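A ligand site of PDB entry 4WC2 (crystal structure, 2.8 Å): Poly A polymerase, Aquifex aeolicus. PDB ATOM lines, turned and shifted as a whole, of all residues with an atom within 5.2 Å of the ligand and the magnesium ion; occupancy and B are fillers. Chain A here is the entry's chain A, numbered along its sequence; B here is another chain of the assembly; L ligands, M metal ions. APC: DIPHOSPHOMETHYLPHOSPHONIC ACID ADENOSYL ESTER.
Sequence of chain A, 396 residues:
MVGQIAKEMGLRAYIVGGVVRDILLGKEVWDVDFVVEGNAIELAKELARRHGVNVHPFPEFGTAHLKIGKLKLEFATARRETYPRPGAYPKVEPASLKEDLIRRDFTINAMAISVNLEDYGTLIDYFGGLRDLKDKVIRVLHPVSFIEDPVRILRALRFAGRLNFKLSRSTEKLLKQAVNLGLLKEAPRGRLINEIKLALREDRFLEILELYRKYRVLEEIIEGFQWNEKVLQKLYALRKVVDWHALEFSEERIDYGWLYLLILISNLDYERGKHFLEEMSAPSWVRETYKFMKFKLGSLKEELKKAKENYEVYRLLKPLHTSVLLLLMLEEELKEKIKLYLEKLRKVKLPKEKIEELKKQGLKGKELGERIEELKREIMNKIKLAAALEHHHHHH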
ATOM      1  N   VAL A  16      -7.906   1.826  -6.137  1.00  0.00           N
ATOM      2  CA  VAL A  16      -6.711   1.117  -6.588  1.00  0.00           C
ATOM      3  C   VAL A  16      -6.798   0.634  -8.042  1.00  0.00           C
ATOM      4  O   VAL A  16      -7.872   0.259  -8.514  1.00  0.00           O
ATOM      5  CB  VAL A  16      -6.425  -0.089  -5.641  1.00  0.00           C
ATOM      6  CG1 VAL A  16      -5.948  -1.310  -6.407  1.00  0.00           C
ATOM      7  CG2 VAL A  16      -5.425   0.308  -4.578  1.00  0.00           C
ATOM      8  N   GLY A  17      -5.661   0.659  -8.728  1.00  0.00           N
ATOM      9  CA  GLY A  17      -5.526  -0.016 -10.011  1.00  0.00           C
ATOM     10  C   GLY A  17      -6.034   0.751 -11.210  1.00  0.00           C
ATOM     11  O   GLY A  17      -5.934   1.980 -11.267  1.00  0.00           O
ATOM     12  N   GLY A  18      -6.581   0.014 -12.174  1.00  0.00           N
ATOM     13  CA  GLY A  18      -7.068   0.583 -13.423  1.00  0.00           C
ATOM     14  C   GLY A  18      -7.979   1.779 -13.241  1.00  0.00           C
ATOM     15  O   GLY A  18      -7.865   2.760 -13.978  1.00  0.00           O
ATOM     16  N   VAL A  19      -8.855   1.704 -12.251  1.00  0.00           N
ATOM     17  CA  VAL A  19      -9.792   2.789 -11.942  1.00  0.00           C
ATOM     18  C   VAL A  19      -9.050   4.120 -11.804  1.00  0.00           C
ATOM     19  O   VAL A  19      -9.485   5.130 -12.346  1.00  0.00           O
ATOM     20  CB  VAL A  19     -10.576   2.516 -10.651  1.00  0.00           C
ATOM     21  CG1 VAL A  19     -11.625   3.607 -10.431  1.00  0.00           C
ATOM     22  CG2 VAL A  19     -11.203   1.135 -10.695  1.00  0.00           C
ATOM     23  N   ARG A  21      -6.024   4.854 -13.050  1.00  0.00           N
ATOM     24  CA  ARG A  21      -5.505   5.167 -14.379  1.00  0.00           C
ATOM     25  C   ARG A  21      -6.558   5.873 -15.238  1.00  0.00           C
ATOM     26  O   ARG A  21      -6.357   6.989 -15.712  1.00  0.00           O
ATOM     27  CB  ARG A  21      -5.020   3.903 -15.086  1.00  0.00           C
ATOM     28  CG  ARG A  21      -4.558   4.113 -16.516  1.00  0.00           C
ATOM     29  CD  ARG A  21      -4.610   2.823 -17.318  1.00  0.00           C
ATOM     30  NE  ARG A  21      -5.975   2.306 -17.440  1.00  0.00           N
ATOM     31  CZ  ARG A  21      -6.329   1.065 -17.130  1.00  0.00           C
ATOM     32  NH1 ARG A  21      -5.430   0.201 -16.688  1.00  0.00           N
ATOM     33  NH2 ARG A  21      -7.593   0.686 -17.283  1.00  0.00           N
ATOM     34  N   ASP A  31     -16.963   0.750 -12.406  1.00  0.00           N
ATOM     35  CA  ASP A  31     -16.383  -0.295 -11.567  1.00  0.00           C
ATOM     36  C   ASP A  31     -15.223   0.283 -10.753  1.00  0.00           C
ATOM     37  O   ASP A  31     -14.245   0.777 -11.316  1.00  0.00           O
ATOM     38  CB  ASP A  31     -15.895  -1.469 -12.427  1.00  0.00           C
ATOM     39  CG  ASP A  31     -17.026  -2.124 -13.201  1.00  0.00           C
ATOM     40  OD1 ASP A  31     -17.593  -3.112 -12.698  1.00  0.00           O
ATOM     41  OD2 ASP A  31     -17.338  -1.653 -14.310  1.00  0.00           O
ATOM     42  N   ASP A  33     -12.415  -0.369  -7.702  1.00  0.00           N
ATOM     43  CA  ASP A  33     -11.703  -1.338  -6.878  1.00  0.00           C
ATOM     44  C   ASP A  33     -11.081  -0.682  -5.649  1.00  0.00           C
ATOM     45  O   ASP A  33     -10.342   0.302  -5.756  1.00  0.00           O
ATOM     46  CB  ASP A  33     -10.611  -2.031  -7.692  1.00  0.00           C
ATOM     47  CG  ASP A  33     -11.181  -2.968  -8.748  1.00  0.00           C
ATOM     48  OD1 ASP A  33     -12.351  -2.762  -9.151  1.00  0.00           O
ATOM     49  OD2 ASP A  33     -10.468  -3.894  -9.165  1.00  0.00           O
ATOM     50  N   ARG A 103       2.559  -6.230  -6.586  1.00  0.00           N
ATOM     51  CA  ARG A 103       2.235  -7.526  -7.160  1.00  0.00           C
ATOM     52  C   ARG A 103       1.419  -7.391  -8.443  1.00  0.00           C
ATOM     53  O   ARG A 103       0.985  -8.389  -9.025  1.00  0.00           O
ATOM     54  CB  ARG A 103       1.482  -8.394  -6.152  1.00  0.00           C
ATOM     55  CG  ARG A 103       0.067  -7.931  -5.886  1.00  0.00           C
ATOM     56  CD  ARG A 103      -0.687  -8.886  -4.979  1.00  0.00           C
ATOM     57  NE  ARG A 103      -2.035  -8.399  -4.670  1.00  0.00           N
ATOM     58  CZ  ARG A 103      -3.081  -8.547  -5.474  1.00  0.00           C
ATOM     59  NH1 ARG A 103      -2.947  -9.164  -6.643  1.00  0.00           N
ATOM     60  NH2 ARG A 103      -4.273  -8.081  -5.106  1.00  0.00           N
ATOM     61  N   ARG A 104       1.210  -6.153  -8.880  1.00  0.00           N
ATOM     62  CA  ARG A 104       0.397  -5.894 -10.065  1.00  0.00           C
ATOM     63  C   ARG A 104       1.255  -5.846 -11.331  1.00  0.00           C
ATOM     64  O   ARG A 104       2.476  -5.969 -11.266  1.00  0.00           O
ATOM     65  CB  ARG A 104      -0.401  -4.601  -9.888  1.00  0.00           C
ATOM     66  CG  ARG A 104      -1.340  -4.681  -8.699  1.00  0.00           C
ATOM     67  CD  ARG A 104      -2.139  -3.424  -8.434  1.00  0.00           C
ATOM     68  NE  ARG A 104      -2.972  -3.625  -7.257  1.00  0.00           N
ATOM     69  CZ  ARG A 104      -4.157  -4.216  -7.274  1.00  0.00           C
ATOM     70  NH1 ARG A 104      -4.677  -4.641  -8.421  1.00  0.00           N
ATOM     71  NH2 ARG A 104      -4.842  -4.371  -6.147  1.00  0.00           N
ATOM     72  N   ASP A 105       0.605  -5.653 -12.483  1.00  0.00           N
ATOM     73  CA  ASP A 105       1.280  -5.836 -13.765  1.00  0.00           C
ATOM     74  C   ASP A 105       2.149  -4.645 -14.169  1.00  0.00           C
ATOM     75  O   ASP A 105       3.372  -4.772 -14.260  1.00  0.00           O
ATOM     76  CB  ASP A 105       0.254  -6.121 -14.869  1.00  0.00           C
ATOM     77  CG  ASP A 105      -0.939  -5.187 -14.816  1.00  0.00           C
ATOM     78  OD1 ASP A 105      -0.868  -4.175 -14.082  1.00  0.00           O
ATOM     79  OD2 ASP A 105      -1.938  -5.464 -15.502  1.00  0.00           O
ATOM     80  N   PHE A 106       1.528  -3.500 -14.403  1.00  0.00           N
ATOM     81  CA  PHE A 106       2.249  -2.344 -14.928  1.00  0.00           C
ATOM     82  C   PHE A 106       2.108  -1.120 -14.044  1.00  0.00           C
ATOM     83  O   PHE A 106       1.109  -0.954 -13.332  1.00  0.00           O
ATOM     84  CB  PHE A 106       1.770  -2.043 -16.351  1.00  0.00           C
ATOM     85  CG  PHE A 106       1.571  -3.272 -17.186  1.00  0.00           C
ATOM     86  CD1 PHE A 106       2.640  -4.064 -17.557  1.00  0.00           C
ATOM     87  CD2 PHE A 106       0.297  -3.645 -17.601  1.00  0.00           C
ATOM     88  CE1 PHE A 106       2.454  -5.199 -18.320  1.00  0.00           C
ATOM     89  CE2 PHE A 106       0.102  -4.770 -18.359  1.00  0.00           C
ATOM     90  CZ  PHE A 106       1.185  -5.552 -18.721  1.00  0.00           C
ATOM     91  N   ASN A 109      -0.918   0.848 -13.811  1.00  0.00           N
ATOM     92  CA  ASN A 109      -1.975   0.144 -13.099  1.00  0.00           C
ATOM     93  C   ASN A 109      -1.679   0.009 -11.611  1.00  0.00           C
ATOM     94  O   ASN A 109      -2.521  -0.483 -10.847  1.00  0.00           O
ATOM     95  CB  ASN A 109      -2.186  -1.244 -13.708  1.00  0.00           C
ATOM     96  CG  ASN A 109      -2.804  -1.188 -15.091  1.00  0.00           C
ATOM     97  OD1 ASN A 109      -3.411  -0.190 -15.471  1.00  0.00           O
ATOM     98  ND2 ASN A 109      -2.662  -2.275 -15.843  1.00  0.00           N
ATOM     99  N   ASP A 149       3.158 -14.213 -14.783  1.00  0.00           N
ATOM    100  CA  ASP A 149       1.850 -14.306 -15.419  1.00  0.00           C
ATOM    101  C   ASP A 149       1.959 -14.024 -16.914  1.00  0.00           C
ATOM    102  O   ASP A 149       1.811 -12.875 -17.349  1.00  0.00           O
ATOM    103  CB  ASP A 149       0.867 -13.336 -14.766  1.00  0.00           C
ATOM    104  CG  ASP A 149      -0.578 -13.713 -15.029  1.00  0.00           C
ATOM    105  OD1 ASP A 149      -0.831 -14.537 -15.930  1.00  0.00           O
ATOM    106  OD2 ASP A 149      -1.466 -13.173 -14.328  1.00  0.00           O
ATOM    107  N   ARG A 152      -0.063 -11.566 -19.057  1.00  0.00           N
ATOM    108  CA  ARG A 152       0.324 -10.161 -19.118  1.00  0.00           C
ATOM    109  C   ARG A 152       0.921  -9.800 -20.472  1.00  0.00           C
ATOM    110  O   ARG A 152       0.762  -8.667 -20.937  1.00  0.00           O
ATOM    111  CB  ARG A 152       1.299  -9.820 -17.994  1.00  0.00           C
ATOM    112  CG  ARG A 152       0.719  -9.955 -16.591  1.00  0.00           C
ATOM    113  CD  ARG A 152       1.762  -9.693 -15.533  1.00  0.00           C
ATOM    114  NE  ARG A 152       1.282 -10.017 -14.189  1.00  0.00           N
ATOM    115  CZ  ARG A 152       2.038  -9.999 -13.095  1.00  0.00           C
ATOM    116  NH1 ARG A 152       3.319  -9.659 -13.170  1.00  0.00           N
ATOM    117  NH2 ARG A 152       1.504 -10.312 -11.922  1.00  0.00           N
ATOM    118  N   ARG A 155      -1.855  -8.660 -22.254  1.00  0.00           N
ATOM    119  CA  ARG A 155      -2.386  -7.476 -21.581  1.00  0.00           C
ATOM    120  C   ARG A 155      -1.623  -6.217 -21.955  1.00  0.00           C
ATOM    121  O   ARG A 155      -2.223  -5.231 -22.402  1.00  0.00           O
ATOM    122  CB  ARG A 155      -2.371  -7.667 -20.060  1.00  0.00           C
ATOM    123  CG  ARG A 155      -3.447  -8.623 -19.541  1.00  0.00           C
ATOM    124  CD  ARG A 155      -3.406  -8.806 -18.028  1.00  0.00           C
ATOM    125  NE  ARG A 155      -3.553  -7.547 -17.309  1.00  0.00           N
ATOM    126  CZ  ARG A 155      -4.713  -6.917 -17.117  1.00  0.00           C
ATOM    127  NH1 ARG A 155      -5.827  -7.427 -17.615  1.00  0.00           N
ATOM    128  NH2 ARG A 155      -4.753  -5.769 -16.448  1.00  0.00           N
ATOM    129  N   ARG A 158      -2.368  -5.075 -25.354  1.00  0.00           N
ATOM    130  CA  ARG A 158      -3.722  -4.541 -25.381  1.00  0.00           C
ATOM    131  C   ARG A 158      -3.719  -3.089 -24.932  1.00  0.00           C
ATOM    132  O   ARG A 158      -4.212  -2.207 -25.635  1.00  0.00           O
ATOM    133  CB  ARG A 158      -4.666  -5.373 -24.507  1.00  0.00           C
ATOM    134  CG  ARG A 158      -6.107  -4.898 -24.526  1.00  0.00           C
ATOM    135  CD  ARG A 158      -7.030  -5.917 -23.873  1.00  0.00           C
ATOM    136  NE  ARG A 158      -6.644  -6.184 -22.492  1.00  0.00           N
ATOM    137  CZ  ARG A 158      -7.303  -5.734 -21.433  1.00  0.00           C
ATOM    138  NH1 ARG A 158      -8.400  -4.993 -21.586  1.00  0.00           N
ATOM    139  NH2 ARG A 158      -6.872  -6.023 -20.214  1.00  0.00           N
ATOM    140  N   PHE A 159      -3.097  -2.852 -23.782  1.00  0.00           N
ATOM    141  CA  PHE A 159      -3.068  -1.493 -23.244  1.00  0.00           C
ATOM    142  C   PHE A 159      -2.339  -0.586 -24.212  1.00  0.00           C
ATOM    143  O   PHE A 159      -2.818   0.493 -24.538  1.00  0.00           O
ATOM    144  CB  PHE A 159      -2.425  -1.475 -21.852  1.00  0.00           C
ATOM    145  CG  PHE A 159      -3.310  -2.065 -20.792  1.00  0.00           C
ATOM    146  CD1 PHE A 159      -4.556  -1.521 -20.516  1.00  0.00           C
ATOM    147  CD2 PHE A 159      -2.894  -3.165 -20.047  1.00  0.00           C
ATOM    148  CE1 PHE A 159      -5.370  -2.056 -19.547  1.00  0.00           C
ATOM    149  CE2 PHE A 159      -3.704  -3.708 -19.074  1.00  0.00           C
ATOM    150  CZ  PHE A 159      -4.947  -3.149 -18.822  1.00  0.00           C
ATOM    151  N   ARG A 162      -4.610   0.114 -26.856  1.00  0.00           N
ATOM    152  CA  ARG A 162      -5.748   0.937 -26.474  1.00  0.00           C
ATOM    153  C   ARG A 162      -5.332   2.388 -26.254  1.00  0.00           C
ATOM    154  O   ARG A 162      -5.961   3.307 -26.774  1.00  0.00           O
ATOM    155  CB  ARG A 162      -6.402   0.399 -25.202  1.00  0.00           C
ATOM    156  CG  ARG A 162      -7.517   1.280 -24.678  1.00  0.00           C
ATOM    157  CD  ARG A 162      -7.760   1.084 -23.198  1.00  0.00           C
ATOM    158  NE  ARG A 162      -8.343  -0.216 -22.892  1.00  0.00           N
ATOM    159  CZ  ARG A 162      -8.708  -0.596 -21.670  1.00  0.00           C
ATOM    160  NH1 ARG A 162      -8.547   0.212 -20.648  1.00  0.00           N
ATOM    161  NH2 ARG A 162      -9.234  -1.800 -21.480  1.00  0.00           N
ATOM    162  N   ARG A 191      -7.493 -18.072 -19.499  1.00  0.00           N
ATOM    163  CA  ARG A 191      -7.101 -16.698 -19.239  1.00  0.00           C
ATOM    164  C   ARG A 191      -6.627 -15.998 -20.516  1.00  0.00           C
ATOM    165  O   ARG A 191      -6.931 -14.823 -20.745  1.00  0.00           O
ATOM    166  CB  ARG A 191      -6.006 -16.655 -18.172  1.00  0.00           C
ATOM    167  CG  ARG A 191      -6.431 -17.234 -16.826  1.00  0.00           C
ATOM    168  CD  ARG A 191      -5.311 -17.164 -15.806  1.00  0.00           C
ATOM    169  NE  ARG A 191      -4.900 -15.781 -15.545  1.00  0.00           N
ATOM    170  CZ  ARG A 191      -3.941 -15.439 -14.687  1.00  0.00           C
ATOM    171  NH1 ARG A 191      -3.298 -16.366 -13.999  1.00  0.00           N
ATOM    172  NH2 ARG A 191      -3.639 -14.154 -14.515  1.00  0.00           N
ATOM    173  N   LEU A 198     -11.278  -9.887 -24.511  1.00  0.00           N
ATOM    174  CA  LEU A 198     -11.215  -8.510 -24.050  1.00  0.00           C
ATOM    175  C   LEU A 198     -10.650  -7.605 -25.128  1.00  0.00           C
ATOM    176  O   LEU A 198     -11.104  -6.483 -25.319  1.00  0.00           O
ATOM    177  CB  LEU A 198     -10.373  -8.403 -22.774  1.00  0.00           C
ATOM    178  CG  LEU A 198     -10.977  -8.975 -21.500  1.00  0.00           C
ATOM    179  CD1 LEU A 198     -10.025  -8.779 -20.328  1.00  0.00           C
ATOM    180  CD2 LEU A 198     -12.319  -8.320 -21.216  1.00  0.00           C
ATOM    181  P     C B  75     -10.965 -12.005  -8.559  1.00  0.00           P
ATOM    182  OP1   C B  75     -11.964 -12.746  -7.743  1.00  0.00           O
ATOM    183  OP2   C B  75     -10.762 -10.552  -8.326  1.00  0.00           O
ATOM    184  O5'   C B  75      -9.558 -12.744  -8.403  1.00  0.00           O
ATOM    185  C5'   C B  75      -8.707 -12.924  -9.529  1.00  0.00           C
ATOM    186  C4'   C B  75      -8.358 -11.608 -10.165  1.00  0.00           C
ATOM    187  O4'   C B  75      -7.137 -11.079  -9.596  1.00  0.00           O
ATOM    188  C3'   C B  75      -8.082 -11.638 -11.661  1.00  0.00           C
ATOM    189  O3'   C B  75      -9.264 -11.687 -12.446  1.00  0.00           O
ATOM    190  C2'   C B  75      -7.248 -10.387 -11.876  1.00  0.00           C
ATOM    191  O2'   C B  75      -8.079  -9.236 -11.951  1.00  0.00           O
ATOM    192  C1'   C B  75      -6.452 -10.321 -10.566  1.00  0.00           C
ATOM    193  N1    C B  75      -5.073 -10.842 -10.705  1.00  0.00           N
ATOM    194  C2    C B  75      -4.045 -10.138 -10.067  1.00  0.00           C
ATOM    195  O2    C B  75      -4.336  -9.139  -9.395  1.00  0.00           O
ATOM    196  N3    C B  75      -2.766 -10.585 -10.172  1.00  0.00           N
ATOM    197  C4    C B  75      -2.492 -11.671 -10.895  1.00  0.00           C
ATOM    198  N4    C B  75      -1.223 -12.066 -10.976  1.00  0.00           N
ATOM    199  C5    C B  75      -3.516 -12.402 -11.576  1.00  0.00           C
ATOM    200  C6    C B  75      -4.769 -11.948 -11.454  1.00  0.00           C
HETATM  201  PG  APC L   1     -10.260  -3.832 -17.689  1.00  0.00           P
HETATM  202  O1G APC L   1     -11.317  -3.248 -16.781  1.00  0.00           O
HETATM  203  O2G APC L   1     -10.257  -5.370 -17.556  1.00  0.00           O
HETATM  204  O3G APC L   1     -10.574  -3.438 -19.155  1.00  0.00           O
HETATM  205  PB  APC L   1      -8.221  -3.408 -15.851  1.00  0.00           P
HETATM  206  O1B APC L   1      -6.831  -2.781 -15.832  1.00  0.00           O
HETATM  207  O2B APC L   1      -9.103  -2.701 -14.836  1.00  0.00           O
HETATM  208  O3B APC L   1      -8.828  -3.257 -17.273  1.00  0.00           O
HETATM  209  PA  APC L   1      -9.109  -5.741 -14.095  1.00  0.00           P
HETATM  210  O1A APC L   1     -10.490  -5.002 -14.137  1.00  0.00           O
HETATM  211  O2A APC L   1      -9.375  -7.309 -14.226  1.00  0.00           O
HETATM  212  C3A APC L   1      -8.048  -5.211 -15.466  1.00  0.00           C
HETATM  213  O5' APC L   1      -8.392  -5.472 -12.689  1.00  0.00           O
HETATM  214  C5' APC L   1      -7.665  -4.323 -12.519  1.00  0.00           C
HETATM  215  C4' APC L   1      -6.537  -4.594 -11.568  1.00  0.00           C
HETATM  216  O4' APC L   1      -6.285  -5.865 -11.547  1.00  0.00           O
HETATM  217  C3' APC L   1      -5.185  -3.798 -12.041  1.00  0.00           C
HETATM  218  O3' APC L   1      -4.496  -3.179 -10.835  1.00  0.00           O
HETATM  219  C2' APC L   1      -4.458  -4.610 -12.568  1.00  0.00           C
HETATM  220  O2' APC L   1      -2.987  -4.302 -12.244  1.00  0.00           O
HETATM  221  C1' APC L   1      -4.870  -6.014 -11.906  1.00  0.00           C
HETATM  222  N9  APC L   1      -4.705  -7.005 -12.761  1.00  0.00           N
HETATM  223  C8  APC L   1      -5.500  -7.562 -13.729  1.00  0.00           C
HETATM  224  N7  APC L   1      -4.769  -8.550 -14.261  1.00  0.00           N
HETATM  225  C5  APC L   1      -3.551  -8.580 -13.625  1.00  0.00           C
HETATM  226  C6  APC L   1      -2.401  -9.374 -13.746  1.00  0.00           C
HETATM  227  N6  APC L   1      -2.290 -10.431 -14.704  1.00  0.00           N
HETATM  228  N1  APC L   1      -1.295  -9.243 -13.021  1.00  0.00           N
HETATM  229  C2  APC L   1      -1.306  -8.240 -12.075  1.00  0.00           C
HETATM  230  N3  APC L   1      -2.427  -7.427 -11.911  1.00  0.00           N
HETATM  231  C4  APC L   1      -3.522  -7.608 -12.685  1.00  0.00           C
HETATM  232 MG    MG M   1     -11.935  -3.327 -14.887  1.00  0.00          MG
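O2' of the ligand is in hydrogen-bond range of OD1 of Asp 105. The guanidinium group (NH1) of Arg 104 lies within hydrogen-bond range of an oxygen (O3') of the ligand (2.8 Å). N6 of the ligand lies within hydrogen-bond range of OD2 of Asp 149. The guanidinium group (NE) of Arg 152 is in hydrogen-bond range of a nitrogen (N1) of the ligand. An oxygen (O3G) of the ligand is in salt-bridge range of the guanidinium group (NH2) of Arg 162, at 3.1 Å. The guanidinium group of Arg 155 is in salt-bridge range of an oxygen (O1B) of the ligand (3.7 Å). The backbone carbonyl oxygen of Asn 109 is in hydrogen-bond range of an oxygen (O3') of the ligand (3.3 Å). NH1 of Arg 21 is in salt-bridge range of O1B of the ligand (3.4 Å). The guanidinium group (NH1) of Arg 158 is in salt-bridge range of an oxygen (O3G) of the ligand (3.6 Å).
O2A of the ligand sits close to O2' of C 75 of chain B (3.3 Å). Gly 17 touches the ligand (CA to O3', 3.4 Å). Arg 103 touches the ligand. Phe 159 touches the ligand. NH2 of Arg 191 touches N6 of the ligand (3.96 Å). Within 4 Å of the ligand: Gly 17, Arg 21, Arg 103, Arg 104, Asp 105, Asn 109, Asp 149, Arg 152, Arg 155, Arg 158, Phe 159, Arg 162, Arg 191 and C 75 of chain B. Along chain A the residues within 4 Å of the ligand span positions 17 to 191. The nearest printed residue that does not touch the ligand is Gly 18 (4.04 Å).
The side-chain carboxylate of Asp 105 is in salt-bridge range of the guanidinium group of Arg 155, 3.0 Å away. The side-chain carboxylate of Asp 105 is in hydrogen-bond range of the side-chain amide nitrogen of Asn 109 (3.2 Å). NH2 of Arg 191 is in salt-bridge range of OD1 of Asp 149 (3.2 Å). The guanidinium group (NH2) of Arg 152 sits at hydrogen-bond distance from N4 of C 75 of chain B. O2 of C 75 of chain B sits at hydrogen-bond distance from the guanidinium group (NH1) of Arg 103 (3.1 Å).
O1G of the ligand binds the magnesium ion, 2.0 Å away. O1A of the ligand binds the magnesium ion.
No residue comes within 4 Å of the magnesium ion.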
